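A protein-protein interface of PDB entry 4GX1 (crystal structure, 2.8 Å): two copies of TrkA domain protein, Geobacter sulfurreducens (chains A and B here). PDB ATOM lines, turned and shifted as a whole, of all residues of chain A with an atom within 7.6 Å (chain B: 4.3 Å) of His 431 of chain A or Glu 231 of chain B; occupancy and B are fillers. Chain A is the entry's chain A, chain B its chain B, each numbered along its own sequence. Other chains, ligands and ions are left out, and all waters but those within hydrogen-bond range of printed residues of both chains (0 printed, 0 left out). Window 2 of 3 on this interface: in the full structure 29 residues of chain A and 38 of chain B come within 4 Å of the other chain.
His 229 of chain B touches Phe 424 of chain A.
Leu 232 of chain B touches Phe 424 of chain A (CD2 to CZ, 3.6 Å).
CD1 of Leu 427 of chain A touches O of Leu 232 of chain B, 3.7 Å away.
CD1 of Leu 235 of chain B touches CD2 of Leu 427 of chain A, at 3.7 Å.
CD2 of Leu 232 of chain B touches CB of Ala 428 of chain A, at 3.8 Å.
His 431 of chain A touches Glu 231 of chain B (NE2 to OE2, 3.6 Å).
CD1 of Leu 232 of chain B touches CD2 of His 431 of chain A, 3.9 Å away.
Of chain B, only Glu 231 and Leu 232 come within 4 Å of His 431 of chain A.
Of chain A, only His 431 comes within 4 Å of Glu 231 of chain B.
Gly 230 of chain B touches none of the printed residues of chain A.
Printed residues of chain B within 4 Å of Phe 424 of chain A: His 229 and Leu 232.
Of the printed residues of chain B, Leu 427 of chain A touches Leu 232 and Leu 235.
Printed residues of chain A within 4 Å of Leu 232 of chain B: Phe 424, Leu 427, Ala 428 and His 431.
Printed residues of chain A within 4 Å of Leu 235 of chain B: Leu 427 (3.7 Å).
The nearest residue of chain A that does not touch Glu 231 of chain B is Leu 427 of chain A (6.8 Å).
The nearest printed residue of chain B that does not touch Phe 424 of chain A is Leu 233 of chain B (4.1 Å).
Hydrophobic or aromatic side chains of chain B that line the printed part of chain A: His 229, Leu 232 and Leu 235.
Of the 15 printed residues of chain A, 4 touch a printed residue of chain B.
Among the printed residues, no Asp or Glu carboxylate lies within 4 Å of a Lys or Arg side-chain nitrogen of the other chain.
No position is printed for both chains.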
ATOM      1  N   PHE A 424      29.429 -27.014   0.443  1.00  0.00           N
ATOM      2  CA  PHE A 424      28.707 -26.220  -0.533  1.00  0.00           C
ATOM      3  C   PHE A 424      27.700 -25.284   0.129  1.00  0.00           C
ATOM      4  O   PHE A 424      27.599 -24.114  -0.234  1.00  0.00           O
ATOM      5  CB  PHE A 424      28.005 -27.138  -1.525  1.00  0.00           C
ATOM      6  CG  PHE A 424      27.586 -26.453  -2.787  1.00  0.00           C
ATOM      7  CD1 PHE A 424      28.533 -25.971  -3.676  1.00  0.00           C
ATOM      8  CD2 PHE A 424      26.248 -26.298  -3.095  1.00  0.00           C
ATOM      9  CE1 PHE A 424      28.154 -25.342  -4.847  1.00  0.00           C
ATOM     10  CE2 PHE A 424      25.867 -25.676  -4.263  1.00  0.00           C
ATOM     11  CZ  PHE A 424      26.824 -25.198  -5.143  1.00  0.00           C
ATOM     12  N   LEU A 425      26.960 -25.803   1.103  1.00  0.00           N
ATOM     13  CA  LEU A 425      25.963 -25.004   1.810  1.00  0.00           C
ATOM     14  C   LEU A 425      26.631 -23.887   2.582  1.00  0.00           C
ATOM     15  O   LEU A 425      26.185 -22.746   2.538  1.00  0.00           O
ATOM     16  CB  LEU A 425      25.144 -25.869   2.769  1.00  0.00           C
ATOM     17  CG  LEU A 425      24.286 -26.954   2.118  1.00  0.00           C
ATOM     18  CD1 LEU A 425      23.617 -27.782   3.192  1.00  0.00           C
ATOM     19  CD2 LEU A 425      23.270 -26.365   1.154  1.00  0.00           C
ATOM     20  N   THR A 426      27.705 -24.226   3.290  1.00  0.00           N
ATOM     21  CA  THR A 426      28.464 -23.242   4.049  1.00  0.00           C
ATOM     22  C   THR A 426      28.924 -22.107   3.146  1.00  0.00           C
ATOM     23  O   THR A 426      28.758 -20.937   3.481  1.00  0.00           O
ATOM     24  CB  THR A 426      29.686 -23.875   4.735  1.00  0.00           C
ATOM     25  OG1 THR A 426      29.251 -24.924   5.606  1.00  0.00           O
ATOM     26  CG2 THR A 426      30.430 -22.835   5.550  1.00  0.00           C
ATOM     27  N   LEU A 427      29.483 -22.463   1.994  1.00  0.00           N
ATOM     28  CA  LEU A 427      29.913 -21.484   1.005  1.00  0.00           C
ATOM     29  C   LEU A 427      28.769 -20.575   0.585  1.00  0.00           C
ATOM     30  O   LEU A 427      28.909 -19.348   0.568  1.00  0.00           O
ATOM     31  CB  LEU A 427      30.451 -22.194  -0.233  1.00  0.00           C
ATOM     32  CG  LEU A 427      31.934 -22.081  -0.570  1.00  0.00           C
ATOM     33  CD1 LEU A 427      32.186 -22.844  -1.856  1.00  0.00           C
ATOM     34  CD2 LEU A 427      32.365 -20.629  -0.695  1.00  0.00           C
ATOM     35  N   ALA A 428      27.641 -21.191   0.237  1.00  0.00           N
ATOM     36  CA  ALA A 428      26.457 -20.465  -0.211  1.00  0.00           C
ATOM     37  C   ALA A 428      25.882 -19.567   0.884  1.00  0.00           C
ATOM     38  O   ALA A 428      25.462 -18.440   0.622  1.00  0.00           O
ATOM     39  CB  ALA A 428      25.403 -21.429  -0.709  1.00  0.00           C
ATOM     40  N   CYS A 429      25.857 -20.067   2.111  1.00  0.00           N
ATOM     41  CA  CYS A 429      25.320 -19.276   3.208  1.00  0.00           C
ATOM     42  C   CYS A 429      26.227 -18.100   3.538  1.00  0.00           C
ATOM     43  O   CYS A 429      25.747 -16.981   3.706  1.00  0.00           O
ATOM     44  CB  CYS A 429      25.057 -20.138   4.447  1.00  0.00           C
ATOM     45  SG  CYS A 429      23.620 -21.221   4.262  1.00  0.00           S
ATOM     46  N   ARG A 430      27.534 -18.346   3.613  1.00  0.00           N
ATOM     47  CA  ARG A 430      28.486 -17.270   3.886  1.00  0.00           C
ATOM     48  C   ARG A 430      28.455 -16.236   2.769  1.00  0.00           C
ATOM     49  O   ARG A 430      28.671 -15.046   2.995  1.00  0.00           O
ATOM     50  CB  ARG A 430      29.904 -17.812   4.057  1.00  0.00           C
ATOM     51  CG  ARG A 430      30.947 -16.758   4.397  1.00  0.00           C
ATOM     52  CD  ARG A 430      31.121 -16.585   5.892  1.00  0.00           C
ATOM     53  NE  ARG A 430      29.891 -16.128   6.516  1.00  0.00           N
ATOM     54  CZ  ARG A 430      29.467 -16.507   7.717  1.00  0.00           C
ATOM     55  NH1 ARG A 430      28.319 -16.031   8.189  1.00  0.00           N
ATOM     56  NH2 ARG A 430      30.177 -17.362   8.443  1.00  0.00           N
ATOM     57  N   HIS A 431      28.176 -16.699   1.559  1.00  0.00           N
ATOM     58  CA  HIS A 431      28.053 -15.800   0.425  1.00  0.00           C
ATOM     59  C   HIS A 431      26.841 -14.867   0.576  1.00  0.00           C
ATOM     60  O   HIS A 431      26.941 -13.665   0.346  1.00  0.00           O
ATOM     61  CB  HIS A 431      27.971 -16.600  -0.875  1.00  0.00           C
ATOM     62  CG  HIS A 431      27.931 -15.749  -2.102  1.00  0.00           C
ATOM     63  ND1 HIS A 431      28.734 -14.642  -2.264  1.00  0.00           N
ATOM     64  CD2 HIS A 431      27.181 -15.839  -3.228  1.00  0.00           C
ATOM     65  CE1 HIS A 431      28.481 -14.086  -3.435  1.00  0.00           C
ATOM     66  NE2 HIS A 431      27.545 -14.794  -4.041  1.00  0.00           N
ATOM     67  N   LEU A 432      25.699 -15.423   0.969  1.00  0.00           N
ATOM     68  CA  LEU A 432      24.487 -14.625   1.123  1.00  0.00           C
ATOM     69  C   LEU A 432      24.558 -13.684   2.318  1.00  0.00           C
ATOM     70  O   LEU A 432      24.209 -12.507   2.209  1.00  0.00           O
ATOM     71  CB  LEU A 432      23.258 -15.520   1.251  1.00  0.00           C
ATOM     72  CG  LEU A 432      22.334 -15.507   0.035  1.00  0.00           C
ATOM     73  CD1 LEU A 432      23.093 -15.915  -1.228  1.00  0.00           C
ATOM     74  CD2 LEU A 432      21.133 -16.415   0.280  1.00  0.00           C
ATOM     75  N   HIS A 433      24.999 -14.211   3.457  1.00  0.00           N
ATOM     76  CA  HIS A 433      25.099 -13.420   4.675  1.00  0.00           C
ATOM     77  C   HIS A 433      26.518 -13.459   5.236  1.00  0.00           C
ATOM     78  O   HIS A 433      26.980 -14.485   5.734  1.00  0.00           O
ATOM     79  CB  HIS A 433      24.086 -13.891   5.715  1.00  0.00           C
ATOM     80  CG  HIS A 433      23.893 -12.926   6.843  1.00  0.00           C
ATOM     81  ND1 HIS A 433      24.940 -12.429   7.589  1.00  0.00           N
ATOM     82  CD2 HIS A 433      22.771 -12.363   7.352  1.00  0.00           C
ATOM     83  CE1 HIS A 433      24.473 -11.603   8.509  1.00  0.00           C
ATOM     84  NE2 HIS A 433      23.159 -11.545   8.386  1.00  0.00           N
ATOM     85  N   SER A 434      27.189 -12.319   5.168  1.00  0.00           N
ATOM     86  CA  SER A 434      28.608 -12.230   5.461  1.00  0.00           C
ATOM     87  C   SER A 434      28.959 -12.472   6.927  1.00  0.00           C
ATOM     88  O   SER A 434      30.113 -12.760   7.247  1.00  0.00           O
ATOM     89  CB  SER A 434      29.134 -10.860   5.038  1.00  0.00           C
ATOM     90  OG  SER A 434      28.726  -9.864   5.959  1.00  0.00           O
ATOM     91  N   ILE A 436      26.464 -14.002   9.518  1.00  0.00           N
ATOM     92  CA  ILE A 436      25.638 -14.941  10.275  1.00  0.00           C
ATOM     93  C   ILE A 436      26.420 -16.156  10.778  1.00  0.00           C
ATOM     94  O   ILE A 436      27.170 -16.787  10.030  1.00  0.00           O
ATOM     95  CB  ILE A 436      24.401 -15.408   9.482  1.00  0.00           C
ATOM     96  CG1 ILE A 436      23.458 -16.202  10.396  1.00  0.00           C
ATOM     97  CG2 ILE A 436      24.818 -16.216   8.253  1.00  0.00           C
ATOM     98  CD1 ILE A 436      22.145 -16.588   9.756  1.00  0.00           C
ATOM     99  N   ILE A 438      27.650 -19.545  11.428  1.00  0.00           N
ATOM    100  CA  ILE A 438      27.490 -20.851  10.798  1.00  0.00           C
ATOM    101  C   ILE A 438      28.278 -21.932  11.531  1.00  0.00           C
ATOM    102  O   ILE A 438      29.502 -21.870  11.613  1.00  0.00           O
ATOM    103  CB  ILE A 438      27.978 -20.841   9.340  1.00  0.00           C
ATOM    104  CG1 ILE A 438      27.098 -19.932   8.478  1.00  0.00           C
ATOM    105  CG2 ILE A 438      28.027 -22.265   8.793  1.00  0.00           C
ATOM    106  CD1 ILE A 438      27.626 -19.725   7.067  1.00  0.00           C
ATOM    107  N   ALA A 454      35.311 -22.377   3.792  1.00  0.00           N
ATOM    108  CA  ALA A 454      34.027 -22.100   3.158  1.00  0.00           C
ATOM    109  C   ALA A 454      33.324 -20.941   3.845  1.00  0.00           C
ATOM    110  O   ALA A 454      32.520 -20.248   3.235  1.00  0.00           O
ATOM    111  CB  ALA A 454      33.150 -23.338   3.158  1.00  0.00           C
ATOM    112  N   GLY A 455      33.637 -20.730   5.118  1.00  0.00           N
ATOM    113  CA  GLY A 455      33.092 -19.606   5.851  1.00  0.00           C
ATOM    114  C   GLY A 455      32.573 -19.964   7.228  1.00  0.00           C
ATOM    115  O   GLY A 455      32.070 -19.098   7.942  1.00  0.00           O
ATOM    116  N   HIS B 229      25.415 -21.608  -9.702  1.00  0.00           N
ATOM    117  CA  HIS B 229      26.484 -22.031  -8.807  1.00  0.00           C
ATOM    118  C   HIS B 229      27.848 -21.555  -9.287  1.00  0.00           C
ATOM    119  O   HIS B 229      28.858 -21.792  -8.632  1.00  0.00           O
ATOM    120  CB  HIS B 229      26.488 -23.553  -8.668  1.00  0.00           C
ATOM    121  CG  HIS B 229      25.250 -24.106  -8.037  1.00  0.00           C
ATOM    122  ND1 HIS B 229      24.692 -25.306  -8.420  1.00  0.00           N
ATOM    123  CD2 HIS B 229      24.468 -23.630  -7.040  1.00  0.00           C
ATOM    124  CE1 HIS B 229      23.618 -25.545  -7.690  1.00  0.00           C
ATOM    125  NE2 HIS B 229      23.461 -24.543  -6.844  1.00  0.00           N
ATOM    126  N   GLY B 230      27.872 -20.887 -10.434  1.00  0.00           N
ATOM    127  CA  GLY B 230      29.107 -20.372 -10.996  1.00  0.00           C
ATOM    128  C   GLY B 230      29.876 -19.434 -10.079  1.00  0.00           C
ATOM    129  O   GLY B 230      31.081 -19.593  -9.908  1.00  0.00           O
ATOM    130  N   GLU B 231      29.190 -18.454  -9.496  1.00  0.00           N
ATOM    131  CA  GLU B 231      29.832 -17.526  -8.569  1.00  0.00           C
ATOM    132  C   GLU B 231      30.374 -18.281  -7.360  1.00  0.00           C
ATOM    133  O   GLU B 231      31.441 -17.960  -6.832  1.00  0.00           O
ATOM    134  CB  GLU B 231      28.839 -16.463  -8.097  1.00  0.00           C
ATOM    135  CG  GLU B 231      27.990 -15.852  -9.199  1.00  0.00           C
ATOM    136  CD  GLU B 231      26.761 -15.119  -8.659  1.00  0.00           C
ATOM    137  OE1 GLU B 231      25.735 -15.068  -9.379  1.00  0.00           O
ATOM    138  OE2 GLU B 231      26.820 -14.599  -7.519  1.00  0.00           O
ATOM    139  N   LEU B 232      29.622 -19.285  -6.926  1.00  0.00           N
ATOM    140  CA  LEU B 232      29.987 -20.093  -5.774  1.00  0.00           C
ATOM    141  C   LEU B 232      31.290 -20.853  -6.015  1.00  0.00           C
ATOM    142  O   LEU B 232      32.113 -21.004  -5.115  1.00  0.00           O
ATOM    143  CB  LEU B 232      28.858 -21.077  -5.472  1.00  0.00           C
ATOM    144  CG  LEU B 232      28.202 -21.024  -4.095  1.00  0.00           C
ATOM    145  CD1 LEU B 232      28.007 -19.592  -3.608  1.00  0.00           C
ATOM    146  CD2 LEU B 232      26.874 -21.761  -4.156  1.00  0.00           C
ATOM    147  N   LEU B 233      31.473 -21.326  -7.241  1.00  0.00           N
ATOM    148  CA  LEU B 233      32.646 -22.111  -7.584  1.00  0.00           C
ATOM    149  C   LEU B 233      33.890 -21.248  -7.824  1.00  0.00           C
ATOM    150  O   LEU B 233      35.016 -21.701  -7.614  1.00  0.00           O
ATOM    151  CB  LEU B 233      32.338 -23.016  -8.777  1.00  0.00           C
ATOM    152  CG  LEU B 233      32.222 -24.509  -8.438  1.00  0.00           C
ATOM    153  CD1 LEU B 233      31.438 -24.729  -7.160  1.00  0.00           C
ATOM    154  CD2 LEU B 233      31.576 -25.275  -9.581  1.00  0.00           C
ATOM    155  N   ARG B 234      33.695 -20.005  -8.256  1.00  0.00           N
ATOM    156  CA  ARG B 234      34.809 -19.066  -8.348  1.00  0.00           C
ATOM    157  C   ARG B 234      35.288 -18.725  -6.946  1.00  0.00           C
ATOM    158  O   ARG B 234      36.487 -18.624  -6.688  1.00  0.00           O
ATOM    159  CB  ARG B 234      34.394 -17.796  -9.081  1.00  0.00           C
ATOM    160  CG  ARG B 234      34.150 -18.001 -10.556  1.00  0.00           C
ATOM    161  CD  ARG B 234      33.789 -16.703 -11.258  1.00  0.00           C
ATOM    162  NE  ARG B 234      33.467 -16.935 -12.663  1.00  0.00           N
ATOM    163  CZ  ARG B 234      34.365 -16.935 -13.643  1.00  0.00           C
ATOM    164  NH1 ARG B 234      35.643 -16.707 -13.370  1.00  0.00           N
ATOM    165  NH2 ARG B 234      33.984 -17.160 -14.895  1.00  0.00           N
ATOM    166  N   LEU B 235      34.327 -18.556  -6.046  1.00  0.00           N
ATOM    167  CA  LEU B 235      34.598 -18.327  -4.638  1.00  0.00           C
ATOM    168  C   LEU B 235      35.465 -19.430  -4.041  1.00  0.00           C
ATOM    169  O   LEU B 235      36.387 -19.151  -3.275  1.00  0.00           O
ATOM    170  CB  LEU B 235      33.283 -18.257  -3.872  1.00  0.00           C
ATOM    171  CG  LEU B 235      33.036 -17.007  -3.040  1.00  0.00           C
ATOM    172  CD1 LEU B 235      31.854 -17.251  -2.123  1.00  0.00           C
ATOM    173  CD2 LEU B 235      34.280 -16.630  -2.252  1.00  0.00           C
